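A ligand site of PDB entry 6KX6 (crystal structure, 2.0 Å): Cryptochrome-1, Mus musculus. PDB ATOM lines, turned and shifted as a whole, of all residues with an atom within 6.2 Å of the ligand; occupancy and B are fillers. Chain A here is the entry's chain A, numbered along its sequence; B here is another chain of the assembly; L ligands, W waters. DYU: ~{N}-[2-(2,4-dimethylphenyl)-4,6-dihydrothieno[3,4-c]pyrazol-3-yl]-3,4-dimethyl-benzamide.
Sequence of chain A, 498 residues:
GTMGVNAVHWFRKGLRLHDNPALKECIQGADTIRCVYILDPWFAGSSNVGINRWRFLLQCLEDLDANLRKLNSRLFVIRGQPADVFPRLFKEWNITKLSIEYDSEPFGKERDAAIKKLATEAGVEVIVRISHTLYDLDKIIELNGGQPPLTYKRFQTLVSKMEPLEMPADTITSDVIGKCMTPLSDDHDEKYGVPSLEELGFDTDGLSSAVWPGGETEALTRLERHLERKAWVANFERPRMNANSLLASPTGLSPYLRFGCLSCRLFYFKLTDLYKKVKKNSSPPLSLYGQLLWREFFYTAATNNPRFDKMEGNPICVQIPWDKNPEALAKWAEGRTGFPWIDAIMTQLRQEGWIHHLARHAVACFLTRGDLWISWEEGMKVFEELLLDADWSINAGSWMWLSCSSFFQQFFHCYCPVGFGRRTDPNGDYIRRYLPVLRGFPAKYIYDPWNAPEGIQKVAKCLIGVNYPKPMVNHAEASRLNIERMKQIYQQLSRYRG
Trp 294 touches the ligand.
Phe 298 touches the ligand.
His 361 touches the ligand (CE1 to C21, 3.9 Å).
Ala 364 touches the ligand.
Phe 383 touches the ligand.
Asp 389 touches the ligand.
Ala 390 touches the ligand (CB to N13, 3.8 Å).
CG2 of Ile 394 touches C11 of the ligand, 3.4 Å away.
OD1 of Asn 395 touches C17 of the ligand, at 3.7 Å.
Trp 399 touches the ligand.
Trp 401 touches the ligand (CE2 to C26, 3.2 Å).
Leu 402 touches the ligand.
Asp 205 of chain B touches the ligand.
Of the 24 residues printed, 16 come within 4 Å of the ligand.
A ring nitrogen (ND1) of His 361 lies within hydrogen-bond range of the backbone carbonyl oxygen (O) of His 357, at 3.0 Å.
The guanidinium group (NH2) of Arg 360 is in salt-bridge range of the side-chain carboxylate (OD2) of Asp 389 (2.7 Å).
The side-chain hydroxyl (OG) of Ser 398 lies within hydrogen-bond range of the backbone carbonyl oxygen (O) of Ile 394 (2.9 Å).
OD2 of Asp 389 lies within hydrogen-bond range of OG of Ser 254.
The indole nitrogen of Trp 399 sits close to the side-chain amide oxygen of Asn 395, 3.2 Å away.
A ring nitrogen (NE2) of His 357 is in hydrogen-bond range of an oxygen (O08) of the ligand, 2.7 Å away.
N13 of the ligand sits at hydrogen-bond distance from NH1 of Arg 360 (2.8 Å).
A nitrogen (N09) of the ligand is in hydrogen-bond range of the side-chain hydroxyl (OG) of Ser 398, 2.8 Å away.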
ATOM      1  N   SER A 254     -24.285 -24.804  -4.616  1.00  0.00           N
ATOM      2  CA  SER A 254     -23.601 -25.607  -5.631  1.00  0.00           C
ATOM      3  C   SER A 254     -24.044 -27.070  -5.650  1.00  0.00           C
ATOM      4  O   SER A 254     -24.353 -27.567  -6.742  1.00  0.00           O
ATOM      5  CB  SER A 254     -22.088 -25.463  -5.483  1.00  0.00           C
ATOM      6  OG  SER A 254     -21.646 -25.569  -4.150  1.00  0.00           O
ATOM      7  N   GLN A 291     -21.897 -18.096 -12.256  1.00  0.00           N
ATOM      8  CA  GLN A 291     -21.952 -19.478 -11.788  1.00  0.00           C
ATOM      9  C   GLN A 291     -22.637 -20.385 -12.803  1.00  0.00           C
ATOM     10  O   GLN A 291     -22.186 -21.511 -13.058  1.00  0.00           O
ATOM     11  CB  GLN A 291     -22.686 -19.524 -10.442  1.00  0.00           C
ATOM     12  CG  GLN A 291     -22.792 -20.911  -9.808  1.00  0.00           C
ATOM     13  CD  GLN A 291     -23.382 -20.858  -8.403  1.00  0.00           C
ATOM     14  OE1 GLN A 291     -23.812 -19.809  -7.927  1.00  0.00           O
ATOM     15  NE2 GLN A 291     -23.415 -22.009  -7.733  1.00  0.00           N
ATOM     16  N   TRP A 294     -20.595 -20.937 -16.497  1.00  0.00           N
ATOM     17  CA  TRP A 294     -19.414 -21.799 -16.491  1.00  0.00           C
ATOM     18  C   TRP A 294     -19.827 -23.264 -16.439  1.00  0.00           C
ATOM     19  O   TRP A 294     -19.180 -24.122 -17.074  1.00  0.00           O
ATOM     20  CB  TRP A 294     -18.502 -21.444 -15.325  1.00  0.00           C
ATOM     21  CG  TRP A 294     -17.481 -20.370 -15.662  1.00  0.00           C
ATOM     22  CD1 TRP A 294     -17.468 -19.088 -15.196  1.00  0.00           C
ATOM     23  CD2 TRP A 294     -16.338 -20.508 -16.523  1.00  0.00           C
ATOM     24  NE1 TRP A 294     -16.386 -18.412 -15.717  1.00  0.00           N
ATOM     25  CE2 TRP A 294     -15.679 -19.264 -16.524  1.00  0.00           C
ATOM     26  CE3 TRP A 294     -15.812 -21.556 -17.287  1.00  0.00           C
ATOM     27  CZ2 TRP A 294     -14.518 -19.036 -17.267  1.00  0.00           C
ATOM     28  CZ3 TRP A 294     -14.655 -21.325 -18.017  1.00  0.00           C
ATOM     29  CH2 TRP A 294     -14.022 -20.083 -18.003  1.00  0.00           C
ATOM     30  N   ARG A 295     -20.892 -23.582 -15.684  1.00  0.00           N
ATOM     31  CA  ARG A 295     -21.544 -24.881 -15.797  1.00  0.00           C
ATOM     32  C   ARG A 295     -21.823 -25.222 -17.249  1.00  0.00           C
ATOM     33  O   ARG A 295     -21.375 -26.248 -17.770  1.00  0.00           O
ATOM     34  CB  ARG A 295     -22.877 -24.880 -15.038  1.00  0.00           C
ATOM     35  CG  ARG A 295     -22.844 -25.144 -13.552  1.00  0.00           C
ATOM     36  CD  ARG A 295     -24.280 -25.061 -13.033  1.00  0.00           C
ATOM     37  NE  ARG A 295     -24.932 -26.376 -12.990  1.00  0.00           N
ATOM     38  CZ  ARG A 295     -26.015 -26.698 -13.693  1.00  0.00           C
ATOM     39  NH1 ARG A 295     -26.572 -25.832 -14.531  1.00  0.00           N
ATOM     40  NH2 ARG A 295     -26.539 -27.915 -13.581  1.00  0.00           N
ATOM     41  N   PHE A 298     -18.872 -26.142 -19.703  1.00  0.00           N
ATOM     42  CA  PHE A 298     -18.236 -27.458 -19.616  1.00  0.00           C
ATOM     43  C   PHE A 298     -19.178 -28.573 -20.071  1.00  0.00           C
ATOM     44  O   PHE A 298     -18.733 -29.559 -20.670  1.00  0.00           O
ATOM     45  CB  PHE A 298     -17.752 -27.708 -18.192  1.00  0.00           C
ATOM     46  CG  PHE A 298     -16.514 -26.934 -17.833  1.00  0.00           C
ATOM     47  CD1 PHE A 298     -15.400 -26.968 -18.651  1.00  0.00           C
ATOM     48  CD2 PHE A 298     -16.468 -26.174 -16.677  1.00  0.00           C
ATOM     49  CE1 PHE A 298     -14.256 -26.260 -18.321  1.00  0.00           C
ATOM     50  CE2 PHE A 298     -15.327 -25.463 -16.333  1.00  0.00           C
ATOM     51  CZ  PHE A 298     -14.218 -25.501 -17.159  1.00  0.00           C
ATOM     52  N   HIS A 357     -13.704 -22.675  -4.187  1.00  0.00           N
ATOM     53  CA  HIS A 357     -13.204 -22.784  -5.553  1.00  0.00           C
ATOM     54  C   HIS A 357     -11.690 -22.573  -5.609  1.00  0.00           C
ATOM     55  O   HIS A 357     -10.983 -23.286  -6.320  1.00  0.00           O
ATOM     56  CB  HIS A 357     -13.913 -21.770  -6.449  1.00  0.00           C
ATOM     57  CG  HIS A 357     -14.918 -22.377  -7.373  1.00  0.00           C
ATOM     58  ND1 HIS A 357     -15.990 -23.126  -6.922  1.00  0.00           N
ATOM     59  CD2 HIS A 357     -15.024 -22.349  -8.721  1.00  0.00           C
ATOM     60  CE1 HIS A 357     -16.701 -23.537  -7.953  1.00  0.00           C
ATOM     61  NE2 HIS A 357     -16.147 -23.074  -9.056  1.00  0.00           N
ATOM     62  N   ARG A 360      -9.875 -25.601  -4.458  1.00  0.00           N
ATOM     63  CA  ARG A 360      -9.786 -26.598  -5.519  1.00  0.00           C
ATOM     64  C   ARG A 360      -8.601 -26.329  -6.431  1.00  0.00           C
ATOM     65  O   ARG A 360      -7.855 -27.259  -6.792  1.00  0.00           O
ATOM     66  CB  ARG A 360     -11.102 -26.634  -6.321  1.00  0.00           C
ATOM     67  CG  ARG A 360     -12.315 -26.926  -5.459  1.00  0.00           C
ATOM     68  CD  ARG A 360     -13.638 -26.796  -6.209  1.00  0.00           C
ATOM     69  NE  ARG A 360     -14.735 -26.527  -5.274  1.00  0.00           N
ATOM     70  CZ  ARG A 360     -15.979 -26.983  -5.405  1.00  0.00           C
ATOM     71  NH1 ARG A 360     -16.314 -27.739  -6.438  1.00  0.00           N
ATOM     72  NH2 ARG A 360     -16.887 -26.678  -4.480  1.00  0.00           N
ATOM     73  N   HIS A 361      -8.395 -25.066  -6.817  1.00  0.00           N
ATOM     74  CA  HIS A 361      -7.191 -24.688  -7.566  1.00  0.00           C
ATOM     75  C   HIS A 361      -5.936 -25.109  -6.829  1.00  0.00           C
ATOM     76  O   HIS A 361      -4.994 -25.641  -7.434  1.00  0.00           O
ATOM     77  CB  HIS A 361      -7.176 -23.182  -7.809  1.00  0.00           C
ATOM     78  CG  HIS A 361      -8.168 -22.701  -8.820  1.00  0.00           C
ATOM     79  ND1 HIS A 361      -9.434 -23.235  -8.939  1.00  0.00           N
ATOM     80  CD2 HIS A 361      -8.089 -21.715  -9.749  1.00  0.00           C
ATOM     81  CE1 HIS A 361     -10.083 -22.605  -9.903  1.00  0.00           C
ATOM     82  NE2 HIS A 361      -9.291 -21.688 -10.409  1.00  0.00           N
ATOM     83  N   ALA A 364      -5.466 -28.916  -6.863  1.00  0.00           N
ATOM     84  CA  ALA A 364      -5.286 -29.390  -8.229  1.00  0.00           C
ATOM     85  C   ALA A 364      -3.891 -29.060  -8.742  1.00  0.00           C
ATOM     86  O   ALA A 364      -3.248 -29.878  -9.418  1.00  0.00           O
ATOM     87  CB  ALA A 364      -6.349 -28.802  -9.150  1.00  0.00           C
ATOM     88  N   PHE A 383     -11.909 -36.382  -6.902  1.00  0.00           N
ATOM     89  CA  PHE A 383     -12.982 -35.400  -6.788  1.00  0.00           C
ATOM     90  C   PHE A 383     -14.340 -36.023  -7.112  1.00  0.00           C
ATOM     91  O   PHE A 383     -15.346 -35.712  -6.469  1.00  0.00           O
ATOM     92  CB  PHE A 383     -12.714 -34.210  -7.707  1.00  0.00           C
ATOM     93  CG  PHE A 383     -11.883 -33.128  -7.089  1.00  0.00           C
ATOM     94  CD1 PHE A 383     -10.990 -33.415  -6.062  1.00  0.00           C
ATOM     95  CD2 PHE A 383     -11.979 -31.820  -7.524  1.00  0.00           C
ATOM     96  CE1 PHE A 383     -10.213 -32.415  -5.487  1.00  0.00           C
ATOM     97  CE2 PHE A 383     -11.213 -30.818  -6.968  1.00  0.00           C
ATOM     98  CZ  PHE A 383     -10.331 -31.119  -5.942  1.00  0.00           C
ATOM     99  N   LEU A 387     -16.447 -34.946  -4.105  1.00  0.00           N
ATOM    100  CA  LEU A 387     -17.024 -33.616  -4.306  1.00  0.00           C
ATOM    101  C   LEU A 387     -18.515 -33.710  -4.588  1.00  0.00           C
ATOM    102  O   LEU A 387     -18.943 -34.475  -5.466  1.00  0.00           O
ATOM    103  CB  LEU A 387     -16.324 -32.893  -5.462  1.00  0.00           C
ATOM    104  CG  LEU A 387     -15.488 -31.636  -5.223  1.00  0.00           C
ATOM    105  CD1 LEU A 387     -15.289 -30.916  -6.554  1.00  0.00           C
ATOM    106  CD2 LEU A 387     -16.137 -30.706  -4.212  1.00  0.00           C
ATOM    107  N   ASP A 389     -20.575 -31.202  -5.709  1.00  0.00           N
ATOM    108  CA  ASP A 389     -21.176 -30.242  -6.627  1.00  0.00           C
ATOM    109  C   ASP A 389     -20.611 -30.276  -8.052  1.00  0.00           C
ATOM    110  O   ASP A 389     -20.974 -29.423  -8.858  1.00  0.00           O
ATOM    111  CB  ASP A 389     -21.052 -28.828  -6.074  1.00  0.00           C
ATOM    112  CG  ASP A 389     -19.614 -28.384  -5.874  1.00  0.00           C
ATOM    113  OD1 ASP A 389     -18.682 -29.182  -6.140  1.00  0.00           O
ATOM    114  OD2 ASP A 389     -19.396 -27.240  -5.434  1.00  0.00           O
ATOM    115  N   ALA A 390     -19.751 -31.230  -8.380  1.00  0.00           N
ATOM    116  CA  ALA A 390     -19.060 -31.231  -9.668  1.00  0.00           C
ATOM    117  C   ALA A 390     -19.475 -32.453 -10.467  1.00  0.00           C
ATOM    118  O   ALA A 390     -19.110 -33.589 -10.125  1.00  0.00           O
ATOM    119  CB  ALA A 390     -17.542 -31.193  -9.486  1.00  0.00           C
ATOM    120  N   ASP A 391     -20.228 -32.230 -11.543  1.00  0.00           N
ATOM    121  CA  ASP A 391     -20.598 -33.311 -12.445  1.00  0.00           C
ATOM    122  C   ASP A 391     -19.389 -33.771 -13.257  1.00  0.00           C
ATOM    123  O   ASP A 391     -18.323 -33.146 -13.265  1.00  0.00           O
ATOM    124  CB  ASP A 391     -21.727 -32.862 -13.376  1.00  0.00           C
ATOM    125  CG  ASP A 391     -23.090 -33.326 -12.906  1.00  0.00           C
ATOM    126  OD1 ASP A 391     -23.177 -34.413 -12.297  1.00  0.00           O
ATOM    127  OD2 ASP A 391     -24.071 -32.589 -13.140  1.00  0.00           O
ATOM    128  N   ILE A 394     -18.033 -31.090 -15.692  1.00  0.00           N
ATOM    129  CA  ILE A 394     -17.378 -29.966 -15.031  1.00  0.00           C
ATOM    130  C   ILE A 394     -16.080 -30.419 -14.365  1.00  0.00           C
ATOM    131  O   ILE A 394     -15.067 -29.723 -14.413  1.00  0.00           O
ATOM    132  CB  ILE A 394     -18.341 -29.318 -14.036  1.00  0.00           C
ATOM    133  CG1 ILE A 394     -19.482 -28.620 -14.779  1.00  0.00           C
ATOM    134  CG2 ILE A 394     -17.604 -28.348 -13.141  1.00  0.00           C
ATOM    135  CD1 ILE A 394     -20.311 -27.695 -13.912  1.00  0.00           C
ATOM    136  N   ASN A 395     -16.109 -31.602 -13.731  1.00  0.00           N
ATOM    137  CA  ASN A 395     -14.912 -32.138 -13.107  1.00  0.00           C
ATOM    138  C   ASN A 395     -13.796 -32.341 -14.120  1.00  0.00           C
ATOM    139  O   ASN A 395     -12.678 -31.837 -13.940  1.00  0.00           O
ATOM    140  CB  ASN A 395     -15.245 -33.458 -12.413  1.00  0.00           C
ATOM    141  CG  ASN A 395     -14.289 -33.773 -11.285  1.00  0.00           C
ATOM    142  OD1 ASN A 395     -13.510 -32.928 -10.863  1.00  0.00           O
ATOM    143  ND2 ASN A 395     -14.344 -35.008 -10.798  1.00  0.00           N
ATOM    144  N   GLY A 397     -13.462 -31.127 -17.211  1.00  0.00           N
ATOM    145  CA  GLY A 397     -13.044 -29.881 -17.831  1.00  0.00           C
ATOM    146  C   GLY A 397     -12.188 -29.033 -16.910  1.00  0.00           C
ATOM    147  O   GLY A 397     -11.195 -28.449 -17.339  1.00  0.00           O
ATOM    148  N   SER A 398     -12.566 -28.953 -15.636  1.00  0.00           N
ATOM    149  CA  SER A 398     -11.783 -28.159 -14.686  1.00  0.00           C
ATOM    150  C   SER A 398     -10.375 -28.738 -14.517  1.00  0.00           C
ATOM    151  O   SER A 398      -9.388 -27.999 -14.545  1.00  0.00           O
ATOM    152  CB  SER A 398     -12.506 -28.075 -13.344  1.00  0.00           C
ATOM    153  OG  SER A 398     -13.719 -27.347 -13.480  1.00  0.00           O
ATOM    154  N   TRP A 399     -10.264 -30.063 -14.391  1.00  0.00           N
ATOM    155  CA  TRP A 399      -8.959 -30.672 -14.163  1.00  0.00           C
ATOM    156  C   TRP A 399      -8.069 -30.537 -15.391  1.00  0.00           C
ATOM    157  O   TRP A 399      -6.850 -30.324 -15.258  1.00  0.00           O
ATOM    158  CB  TRP A 399      -9.113 -32.137 -13.775  1.00  0.00           C
ATOM    159  CG  TRP A 399      -9.360 -32.322 -12.317  1.00  0.00           C
ATOM    160  CD1 TRP A 399     -10.567 -32.484 -11.702  1.00  0.00           C
ATOM    161  CD2 TRP A 399      -8.378 -32.335 -11.281  1.00  0.00           C
ATOM    162  NE1 TRP A 399     -10.399 -32.611 -10.343  1.00  0.00           N
ATOM    163  CE2 TRP A 399      -9.059 -32.524 -10.060  1.00  0.00           C
ATOM    164  CE3 TRP A 399      -6.987 -32.219 -11.261  1.00  0.00           C
ATOM    165  CZ2 TRP A 399      -8.394 -32.584  -8.836  1.00  0.00           C
ATOM    166  CZ3 TRP A 399      -6.327 -32.282 -10.046  1.00  0.00           C
ATOM    167  CH2 TRP A 399      -7.034 -32.465  -8.850  1.00  0.00           C
ATOM    168  N   TRP A 401      -8.300 -28.040 -17.519  1.00  0.00           N
ATOM    169  CA  TRP A 401      -7.962 -26.619 -17.545  1.00  0.00           C
ATOM    170  C   TRP A 401      -6.807 -26.313 -16.605  1.00  0.00           C
ATOM    171  O   TRP A 401      -5.809 -25.696 -17.002  1.00  0.00           O
ATOM    172  CB  TRP A 401      -9.190 -25.790 -17.164  1.00  0.00           C
ATOM    173  CG  TRP A 401      -9.062 -24.335 -17.459  1.00  0.00           C
ATOM    174  CD1 TRP A 401      -8.140 -23.469 -16.953  1.00  0.00           C
ATOM    175  CD2 TRP A 401      -9.912 -23.556 -18.329  1.00  0.00           C
ATOM    176  NE1 TRP A 401      -8.351 -22.210 -17.450  1.00  0.00           N
ATOM    177  CE2 TRP A 401      -9.418 -22.228 -18.301  1.00  0.00           C
ATOM    178  CE3 TRP A 401     -11.015 -23.846 -19.121  1.00  0.00           C
ATOM    179  CZ2 TRP A 401     -10.014 -21.208 -19.028  1.00  0.00           C
ATOM    180  CZ3 TRP A 401     -11.603 -22.825 -19.853  1.00  0.00           C
ATOM    181  CH2 TRP A 401     -11.097 -21.521 -19.809  1.00  0.00           C
ATOM    182  N   LEU A 402      -6.922 -26.731 -15.348  1.00  0.00           N
ATOM    183  CA  LEU A 402      -5.963 -26.323 -14.332  1.00  0.00           C
ATOM    184  C   LEU A 402      -4.622 -27.031 -14.487  1.00  0.00           C
ATOM    185  O   LEU A 402      -3.617 -26.544 -13.952  1.00  0.00           O
ATOM    186  CB  LEU A 402      -6.534 -26.570 -12.935  1.00  0.00           C
ATOM    187  CG  LEU A 402      -7.788 -25.756 -12.619  1.00  0.00           C
ATOM    188  CD1 LEU A 402      -8.400 -26.211 -11.301  1.00  0.00           C
ATOM    189  CD2 LEU A 402      -7.462 -24.275 -12.580  1.00  0.00           C
ATOM    190  N   THR B 204      -9.649 -15.316 -11.429  1.00  0.00           N
ATOM    191  CA  THR B 204      -8.909 -15.261 -12.684  1.00  0.00           C
ATOM    192  C   THR B 204      -9.507 -16.156 -13.766  1.00  0.00           C
ATOM    193  O   THR B 204      -8.893 -16.340 -14.816  1.00  0.00           O
ATOM    194  CB  THR B 204      -7.451 -15.638 -12.464  1.00  0.00           C
ATOM    195  OG1 THR B 204      -7.382 -16.913 -11.794  1.00  0.00           O
ATOM    196  CG2 THR B 204      -6.758 -14.590 -11.592  1.00  0.00           C
ATOM    197  N   ASP B 205     -10.695 -16.731 -13.527  1.00  0.00           N
ATOM    198  CA  ASP B 205     -11.268 -17.691 -14.458  1.00  0.00           C
ATOM    199  C   ASP B 205     -11.501 -17.051 -15.819  1.00  0.00           C
ATOM    200  O   ASP B 205     -12.231 -16.071 -15.934  1.00  0.00           O
ATOM    201  CB  ASP B 205     -12.578 -18.240 -13.891  1.00  0.00           C
ATOM    202  CG  ASP B 205     -12.367 -19.096 -12.654  1.00  0.00           C
ATOM    203  OD1 ASP B 205     -11.257 -19.648 -12.492  1.00  0.00           O
ATOM    204  OD2 ASP B 205     -13.316 -19.219 -11.856  1.00  0.00           O
ATOM    205  N   GLY B 206     -10.857 -17.611 -16.849  1.00  0.00           N
ATOM    206  CA  GLY B 206     -11.025 -17.125 -18.200  1.00  0.00           C
ATOM    207  C   GLY B 206     -10.169 -15.930 -18.562  1.00  0.00           C
ATOM    208  O   GLY B 206     -10.265 -15.443 -19.694  1.00  0.00           O
HETATM  209  C10 DYU L   1     -15.926 -26.079 -11.023  1.00  0.00           C
HETATM  210  C15 DYU L   1     -14.021 -27.498 -10.056  1.00  0.00           C
HETATM  211  C17 DYU L   1     -12.542 -29.390 -10.176  1.00  0.00           C
HETATM  212  C20 DYU L   1     -12.921 -26.660  -9.860  1.00  0.00           C
HETATM  213  C21 DYU L   1     -13.052 -25.153  -9.663  1.00  0.00           C
HETATM  214  C22 DYU L   1     -10.041 -29.153  -9.945  1.00  0.00           C
HETATM  215  C26 DYU L   1     -11.401 -21.558 -15.843  1.00  0.00           C
HETATM  216  C01 DYU L   1     -13.015 -23.907 -13.367  1.00  0.00           C
HETATM  217  C02 DYU L   1     -12.080 -23.348 -14.209  1.00  0.00           C
HETATM  218  C03 DYU L   1     -12.408 -22.201 -14.898  1.00  0.00           C
HETATM  219  C04 DYU L   1     -13.635 -21.604 -14.743  1.00  0.00           C
HETATM  220  C05 DYU L   1     -14.582 -22.154 -13.899  1.00  0.00           C
HETATM  221  C06 DYU L   1     -14.261 -23.318 -13.223  1.00  0.00           C
HETATM  222  C07 DYU L   1     -15.236 -23.964 -12.245  1.00  0.00           C
HETATM  223  C11 DYU L   1     -17.244 -25.939 -10.769  1.00  0.00           C
HETATM  224  C12 DYU L   1     -17.592 -26.944  -9.569  1.00  0.00           C
HETATM  225  C16 DYU L   1     -13.811 -28.854 -10.218  1.00  0.00           C
HETATM  226  C18 DYU L   1     -11.452 -28.565  -9.981  1.00  0.00           C
HETATM  227  C19 DYU L   1     -11.640 -27.205  -9.821  1.00  0.00           C
HETATM  228  C23 DYU L   1     -19.147 -26.839  -9.227  1.00  0.00           C
HETATM  229  C25 DYU L   1     -18.572 -25.163 -11.208  1.00  0.00           C
HETATM  230  C27 DYU L   1     -10.718 -24.013 -14.383  1.00  0.00           C
HETATM  231  N09 DYU L   1     -15.100 -25.382 -11.991  1.00  0.00           N
HETATM  232  N13 DYU L   1     -16.474 -27.562  -9.245  1.00  0.00           N
HETATM  233  N14 DYU L   1     -15.399 -27.039 -10.112  1.00  0.00           N
HETATM  234  O08 DYU L   1     -16.063 -23.302 -11.703  1.00  0.00           O
HETATM  235  S24 DYU L   1     -19.832 -26.046 -10.541  1.00  0.00           S
HETATM  236  O   HOH W   1     -19.171 -24.725  -6.677  1.00  0.00           O
HETATM  237  O   HOH W   2     -22.788 -27.055  -9.039  1.00  0.00           O
